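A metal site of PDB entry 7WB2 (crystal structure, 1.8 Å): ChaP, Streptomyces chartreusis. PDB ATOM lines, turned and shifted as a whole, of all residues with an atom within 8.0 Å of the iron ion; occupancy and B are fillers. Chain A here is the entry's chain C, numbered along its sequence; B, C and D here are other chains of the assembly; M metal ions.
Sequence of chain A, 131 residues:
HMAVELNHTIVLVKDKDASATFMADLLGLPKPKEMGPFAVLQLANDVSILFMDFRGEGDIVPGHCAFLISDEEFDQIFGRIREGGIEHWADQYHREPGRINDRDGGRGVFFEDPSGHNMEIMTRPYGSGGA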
ATOM      1  N   ALA A   3     -17.782  11.655 -29.877  1.00  0.00           N
ATOM      2  CA  ALA A   3     -19.161  11.752 -29.414  1.00  0.00           C
ATOM      3  C   ALA A   3     -20.084  12.483 -30.370  1.00  0.00           C
ATOM      4  O   ALA A   3     -21.299  12.466 -30.150  1.00  0.00           O
ATOM      5  CB  ALA A   3     -19.220  12.435 -28.042  1.00  0.00           C
ATOM      6  N   VAL A   4     -19.570  13.143 -31.402  1.00  0.00           N
ATOM      7  CA  VAL A   4     -20.429  13.934 -32.275  1.00  0.00           C
ATOM      8  C   VAL A   4     -21.348  13.016 -33.055  1.00  0.00           C
ATOM      9  O   VAL A   4     -20.913  12.006 -33.607  1.00  0.00           O
ATOM     10  CB  VAL A   4     -19.598  14.803 -33.229  1.00  0.00           C
ATOM     11  CG1 VAL A   4     -20.472  15.861 -33.878  1.00  0.00           C
ATOM     12  CG2 VAL A   4     -18.486  15.463 -32.452  1.00  0.00           C
ATOM     13  N   GLU A   5     -22.625  13.414 -33.162  1.00  0.00           N
ATOM     14  CA  GLU A   5     -23.632  12.667 -33.886  1.00  0.00           C
ATOM     15  C   GLU A   5     -24.119  13.454 -35.105  1.00  0.00           C
ATOM     16  O   GLU A   5     -24.141  14.687 -35.104  1.00  0.00           O
ATOM     17  CB  GLU A   5     -24.833  12.357 -32.983  1.00  0.00           C
ATOM     18  CG  GLU A   5     -24.408  11.757 -31.653  1.00  0.00           C
ATOM     19  CD  GLU A   5     -25.558  11.310 -30.794  1.00  0.00           C
ATOM     20  OE1 GLU A   5     -25.300  10.751 -29.714  1.00  0.00           O
ATOM     21  OE2 GLU A   5     -26.727  11.514 -31.207  1.00  0.00           O
ATOM     22  N   LEU A   6     -24.481  12.722 -36.157  1.00  0.00           N
ATOM     23  CA  LEU A   6     -25.176  13.310 -37.291  1.00  0.00           C
ATOM     24  C   LEU A   6     -26.660  13.328 -36.951  1.00  0.00           C
ATOM     25  O   LEU A   6     -27.298  12.284 -36.826  1.00  0.00           O
ATOM     26  CB  LEU A   6     -24.892  12.520 -38.570  1.00  0.00           C
ATOM     27  CG  LEU A   6     -25.540  13.080 -39.828  1.00  0.00           C
ATOM     28  CD1 LEU A   6     -24.894  14.396 -40.234  1.00  0.00           C
ATOM     29  CD2 LEU A   6     -25.410  12.064 -40.949  1.00  0.00           C
ATOM     30  N   ASN A   7     -27.203  14.535 -36.781  1.00  0.00           N
ATOM     31  CA  ASN A   7     -28.577  14.660 -36.296  1.00  0.00           C
ATOM     32  C   ASN A   7     -29.589  14.726 -37.427  1.00  0.00           C
ATOM     33  O   ASN A   7     -30.693  14.194 -37.299  1.00  0.00           O
ATOM     34  CB  ASN A   7     -28.714  15.891 -35.408  1.00  0.00           C
ATOM     35  CG  ASN A   7     -30.114  16.070 -34.890  1.00  0.00           C
ATOM     36  OD1 ASN A   7     -30.918  16.764 -35.516  1.00  0.00           O
ATOM     37  ND2 ASN A   7     -30.425  15.416 -33.773  1.00  0.00           N
ATOM     38  N   ASN A  45     -31.523   5.685 -35.189  1.00  0.00           N
ATOM     39  CA  ASN A  45     -30.284   6.083 -34.530  1.00  0.00           C
ATOM     40  C   ASN A  45     -30.122   7.607 -34.419  1.00  0.00           C
ATOM     41  O   ASN A  45     -29.081   8.148 -34.776  1.00  0.00           O
ATOM     42  CB  ASN A  45     -29.095   5.426 -35.222  1.00  0.00           C
ATOM     43  CG  ASN A  45     -29.071   5.625 -36.755  1.00  0.00           C
ATOM     44  OD1 ASN A  45     -30.111   5.582 -37.414  1.00  0.00           O
ATOM     45  ND2 ASN A  45     -27.867   5.783 -37.303  1.00  0.00           N
ATOM     46  N   ASP A  46     -31.139   8.295 -33.894  1.00  0.00           N
ATOM     47  CA  ASP A  46     -31.060   9.728 -33.567  1.00  0.00           C
ATOM     48  C   ASP A  46     -30.673  10.561 -34.789  1.00  0.00           C
ATOM     49  O   ASP A  46     -29.871  11.487 -34.703  1.00  0.00           O
ATOM     50  CB  ASP A  46     -30.097   9.971 -32.398  1.00  0.00           C
ATOM     51  CG  ASP A  46     -30.372  11.271 -31.654  1.00  0.00           C
ATOM     52  OD1 ASP A  46     -31.356  11.957 -32.019  1.00  0.00           O
ATOM     53  OD2 ASP A  46     -29.610  11.629 -30.708  1.00  0.00           O
ATOM     54  N   VAL A  47     -31.260  10.228 -35.945  1.00  0.00           N
ATOM     55  CA  VAL A  47     -30.949  10.908 -37.197  1.00  0.00           C
ATOM     56  C   VAL A  47     -32.197  10.946 -38.079  1.00  0.00           C
ATOM     57  O   VAL A  47     -33.005  10.019 -38.072  1.00  0.00           O
ATOM     58  CB  VAL A  47     -29.789  10.206 -37.952  1.00  0.00           C
ATOM     59  CG1 VAL A  47     -30.169   8.797 -38.313  1.00  0.00           C
ATOM     60  CG2 VAL A  47     -29.422  10.985 -39.196  1.00  0.00           C
ATOM     61  N   ALA B   3     -30.302   1.112 -31.084  1.00  0.00           N
ATOM     62  CA  ALA B   3     -30.083   2.532 -31.292  1.00  0.00           C
ATOM     63  C   ALA B   3     -30.497   3.393 -30.109  1.00  0.00           C
ATOM     64  O   ALA B   3     -30.367   4.619 -30.191  1.00  0.00           O
ATOM     65  CB  ALA B   3     -30.789   3.007 -32.579  1.00  0.00           C
ATOM     66  N   VAL B   4     -31.049   2.790 -29.050  1.00  0.00           N
ATOM     67  CA  VAL B   4     -31.588   3.534 -27.905  1.00  0.00           C
ATOM     68  C   VAL B   4     -30.444   4.199 -27.158  1.00  0.00           C
ATOM     69  O   VAL B   4     -29.420   3.570 -26.893  1.00  0.00           O
ATOM     70  CB  VAL B   4     -32.373   2.588 -26.971  1.00  0.00           C
ATOM     71  CG1 VAL B   4     -32.797   3.312 -25.693  1.00  0.00           C
ATOM     72  CG2 VAL B   4     -33.584   1.970 -27.690  1.00  0.00           C
ATOM     73  N   GLU B   5     -30.631   5.466 -26.790  1.00  0.00           N
ATOM     74  CA  GLU B   5     -29.610   6.199 -26.068  1.00  0.00           C
ATOM     75  C   GLU B   5     -30.083   6.551 -24.658  1.00  0.00           C
ATOM     76  O   GLU B   5     -31.282   6.732 -24.432  1.00  0.00           O
ATOM     77  CB  GLU B   5     -29.229   7.482 -26.825  1.00  0.00           C
ATOM     78  CG  GLU B   5     -28.717   7.215 -28.234  1.00  0.00           C
ATOM     79  CD  GLU B   5     -28.368   8.493 -28.946  1.00  0.00           C
ATOM     80  OE1 GLU B   5     -28.544   9.574 -28.338  1.00  0.00           O
ATOM     81  OE2 GLU B   5     -27.872   8.409 -30.077  1.00  0.00           O
ATOM     82  N   LEU B   6     -29.133   6.624 -23.737  1.00  0.00           N
ATOM     83  CA  LEU B   6     -29.409   7.167 -22.412  1.00  0.00           C
ATOM     84  C   LEU B   6     -29.277   8.684 -22.490  1.00  0.00           C
ATOM     85  O   LEU B   6     -28.173   9.205 -22.626  1.00  0.00           O
ATOM     86  CB  LEU B   6     -28.485   6.558 -21.359  1.00  0.00           C
ATOM     87  CG  LEU B   6     -28.722   7.113 -19.958  1.00  0.00           C
ATOM     88  CD1 LEU B   6     -30.111   6.765 -19.484  1.00  0.00           C
ATOM     89  CD2 LEU B   6     -27.689   6.569 -19.010  1.00  0.00           C
ATOM     90  N   ASN B   7     -30.405   9.397 -22.368  1.00  0.00           N
ATOM     91  CA  ASN B   7     -30.429  10.850 -22.607  1.00  0.00           C
ATOM     92  C   ASN B   7     -30.182  11.660 -21.345  1.00  0.00           C
ATOM     93  O   ASN B   7     -29.516  12.708 -21.394  1.00  0.00           O
ATOM     94  CB  ASN B   7     -31.755  11.272 -23.242  1.00  0.00           C
ATOM     95  CG  ASN B   7     -31.812  12.759 -23.577  1.00  0.00           C
ATOM     96  OD1 ASN B   7     -32.406  13.551 -22.852  1.00  0.00           O
ATOM     97  ND2 ASN B   7     -31.161  13.148 -24.686  1.00  0.00           N
ATOM     98  N   ALA B  44     -20.359  14.777 -23.053  1.00  0.00           N
ATOM     99  CA  ALA B  44     -20.245  14.939 -24.495  1.00  0.00           C
ATOM    100  C   ALA B  44     -21.095  13.950 -25.289  1.00  0.00           C
ATOM    101  O   ALA B  44     -21.531  14.281 -26.395  1.00  0.00           O
ATOM    102  CB  ALA B  44     -18.780  14.819 -24.915  1.00  0.00           C
ATOM    103  N   ASN B  45     -21.377  12.770 -24.727  1.00  0.00           N
ATOM    104  CA  ASN B  45     -22.037  11.703 -25.488  1.00  0.00           C
ATOM    105  C   ASN B  45     -23.557  11.765 -25.364  1.00  0.00           C
ATOM    106  O   ASN B  45     -24.211  10.781 -25.044  1.00  0.00           O
ATOM    107  CB  ASN B  45     -21.486  10.339 -25.069  1.00  0.00           C
ATOM    108  CG  ASN B  45     -21.463  10.128 -23.540  1.00  0.00           C
ATOM    109  OD1 ASN B  45     -21.208  11.060 -22.783  1.00  0.00           O
ATOM    110  ND2 ASN B  45     -21.636   8.882 -23.101  1.00  0.00           N
ATOM    111  N   ASP B  46     -24.127  12.952 -25.624  1.00  0.00           N
ATOM    112  CA  ASP B  46     -25.585  13.128 -25.713  1.00  0.00           C
ATOM    113  C   ASP B  46     -26.289  12.613 -24.449  1.00  0.00           C
ATOM    114  O   ASP B  46     -27.317  11.941 -24.516  1.00  0.00           O
ATOM    115  CB  ASP B  46     -26.158  12.460 -26.961  1.00  0.00           C
ATOM    116  CG  ASP B  46     -27.486  13.057 -27.383  1.00  0.00           C
ATOM    117  OD1 ASP B  46     -27.944  14.012 -26.732  1.00  0.00           O
ATOM    118  OD2 ASP B  46     -28.081  12.555 -28.368  1.00  0.00           O
ATOM    119  N   VAL B  47     -25.705  12.917 -23.287  1.00  0.00           N
ATOM    120  CA  VAL B  47     -26.273  12.516 -22.006  1.00  0.00           C
ATOM    121  C   VAL B  47     -25.924  13.567 -20.969  1.00  0.00           C
ATOM    122  O   VAL B  47     -24.844  14.175 -21.007  1.00  0.00           O
ATOM    123  CB  VAL B  47     -25.770  11.122 -21.572  1.00  0.00           C
ATOM    124  CG1 VAL B  47     -24.294  11.151 -21.263  1.00  0.00           C
ATOM    125  CG2 VAL B  47     -26.572  10.609 -20.371  1.00  0.00           C
ATOM    126  N   ALA C  44     -20.821   9.319 -34.166  1.00  0.00           N
ATOM    127  CA  ALA C  44     -21.024   8.476 -32.992  1.00  0.00           C
ATOM    128  C   ALA C  44     -22.318   7.668 -33.053  1.00  0.00           C
ATOM    129  O   ALA C  44     -22.404   6.598 -32.436  1.00  0.00           O
ATOM    130  CB  ALA C  44     -21.000   9.319 -31.720  1.00  0.00           C
ATOM    131  N   ASN C  45     -23.348   8.165 -33.755  1.00  0.00           N
ATOM    132  CA  ASN C  45     -24.630   7.466 -33.749  1.00  0.00           C
ATOM    133  C   ASN C  45     -24.757   6.486 -34.920  1.00  0.00           C
ATOM    134  O   ASN C  45     -25.799   6.401 -35.580  1.00  0.00           O
ATOM    135  CB  ASN C  45     -25.785   8.456 -33.735  1.00  0.00           C
ATOM    136  CG  ASN C  45     -25.650   9.546 -34.787  1.00  0.00           C
ATOM    137  OD1 ASN C  45     -24.560   9.967 -35.110  1.00  0.00           O
ATOM    138  ND2 ASN C  45     -26.780  10.040 -35.269  1.00  0.00           N
ATOM    139  N   LEU C  68     -24.729  17.172 -33.994  1.00  0.00           N
ATOM    140  CA  LEU C  68     -25.112  17.419 -32.609  1.00  0.00           C
ATOM    141  C   LEU C  68     -23.919  17.263 -31.678  1.00  0.00           C
ATOM    142  O   LEU C  68     -23.242  16.233 -31.681  1.00  0.00           O
ATOM    143  CB  LEU C  68     -26.220  16.470 -32.171  1.00  0.00           C
ATOM    144  CG  LEU C  68     -26.683  16.725 -30.738  1.00  0.00           C
ATOM    145  CD1 LEU C  68     -27.681  17.840 -30.630  1.00  0.00           C
ATOM    146  CD2 LEU C  68     -27.263  15.413 -30.216  1.00  0.00           C
ATOM    147  N   ARG C 124     -28.376  20.375 -28.028  1.00  0.00           N
ATOM    148  CA  ARG C 124     -29.705  19.935 -27.575  1.00  0.00           C
ATOM    149  C   ARG C 124     -29.615  19.666 -26.081  1.00  0.00           C
ATOM    150  O   ARG C 124     -29.629  18.516 -25.635  1.00  0.00           O
ATOM    151  CB  ARG C 124     -30.163  18.685 -28.336  1.00  0.00           C
ATOM    152  N   ALA D  44     -26.780   3.015 -26.775  1.00  0.00           N
ATOM    153  CA  ALA D  44     -26.079   3.251 -28.036  1.00  0.00           C
ATOM    154  C   ALA D  44     -25.093   4.410 -27.933  1.00  0.00           C
ATOM    155  O   ALA D  44     -24.126   4.455 -28.702  1.00  0.00           O
ATOM    156  CB  ALA D  44     -27.078   3.499 -29.162  1.00  0.00           C
ATOM    157  N   ASN D  45     -25.313   5.359 -27.029  1.00  0.00           N
ATOM    158  CA  ASN D  45     -24.444   6.543 -26.973  1.00  0.00           C
ATOM    159  C   ASN D  45     -23.296   6.343 -25.991  1.00  0.00           C
ATOM    160  O   ASN D  45     -22.961   7.237 -25.221  1.00  0.00           O
ATOM    161  CB  ASN D  45     -25.252   7.784 -26.641  1.00  0.00           C
ATOM    162  CG  ASN D  45     -26.095   7.626 -25.381  1.00  0.00           C
ATOM    163  OD1 ASN D  45     -26.625   6.540 -25.102  1.00  0.00           O
ATOM    164  ND2 ASN D  45     -26.249   8.710 -24.618  1.00  0.00           N
ATOM    165  N   LEU D  68     -33.983   7.948 -24.959  1.00  0.00           N
ATOM    166  CA  LEU D  68     -34.310   8.635 -26.193  1.00  0.00           C
ATOM    167  C   LEU D  68     -34.430   7.629 -27.310  1.00  0.00           C
ATOM    168  O   LEU D  68     -33.516   6.823 -27.541  1.00  0.00           O
ATOM    169  CB  LEU D  68     -33.239   9.687 -26.519  1.00  0.00           C
HETATM  170 FE    FE M   1     -28.037  11.142 -29.689  1.00  0.00          FE
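The backbone carbonyl oxygen of Asp 46 of chain B sits at hydrogen-bond distance from the side-chain amide nitrogen of Asn 45 of chain D (3.4 Å). ND2 of Asn 45 of chain C sits at hydrogen-bond distance from O of Asp 46 of chain A (3.5 Å). The backbone NH (N) of Leu 68 of chain C is in hydrogen-bond range of the backbone carbonyl oxygen (O) of Glu 5 of chain A (2.8 Å). O of Glu 5 of chain B lies within hydrogen-bond range of N of Leu 68 of chain D, at 3.0 Å.
Of the 24 residues printed, 4 come within 4 Å of the iron ion. Along chain A the residues within 4 Å of the iron ion span positions 5 to 46.
The iron ion is bound by OD2 of Asp 46 of chain B (1.9 Å). The side-chain carboxylate (OD2) of Asp 46 of chain A binds the iron ion (1.9 Å). The side-chain carboxylate (OE2) of Glu 5 of chain A is bound to the iron ion (2.0 Å). The iron ion is bound by the side-chain carboxylate (OE1) of Glu 5 of chain B (2.1 Å). The iron ion has four donor atoms within binding distance. Slightly farther from the iron ion lies the side-chain carboxylate (OE1) of Glu 5 of chain A (2.8 Å). Slightly farther from the iron ion lies OE2 of Glu 5 of chain B (2.8 Å).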
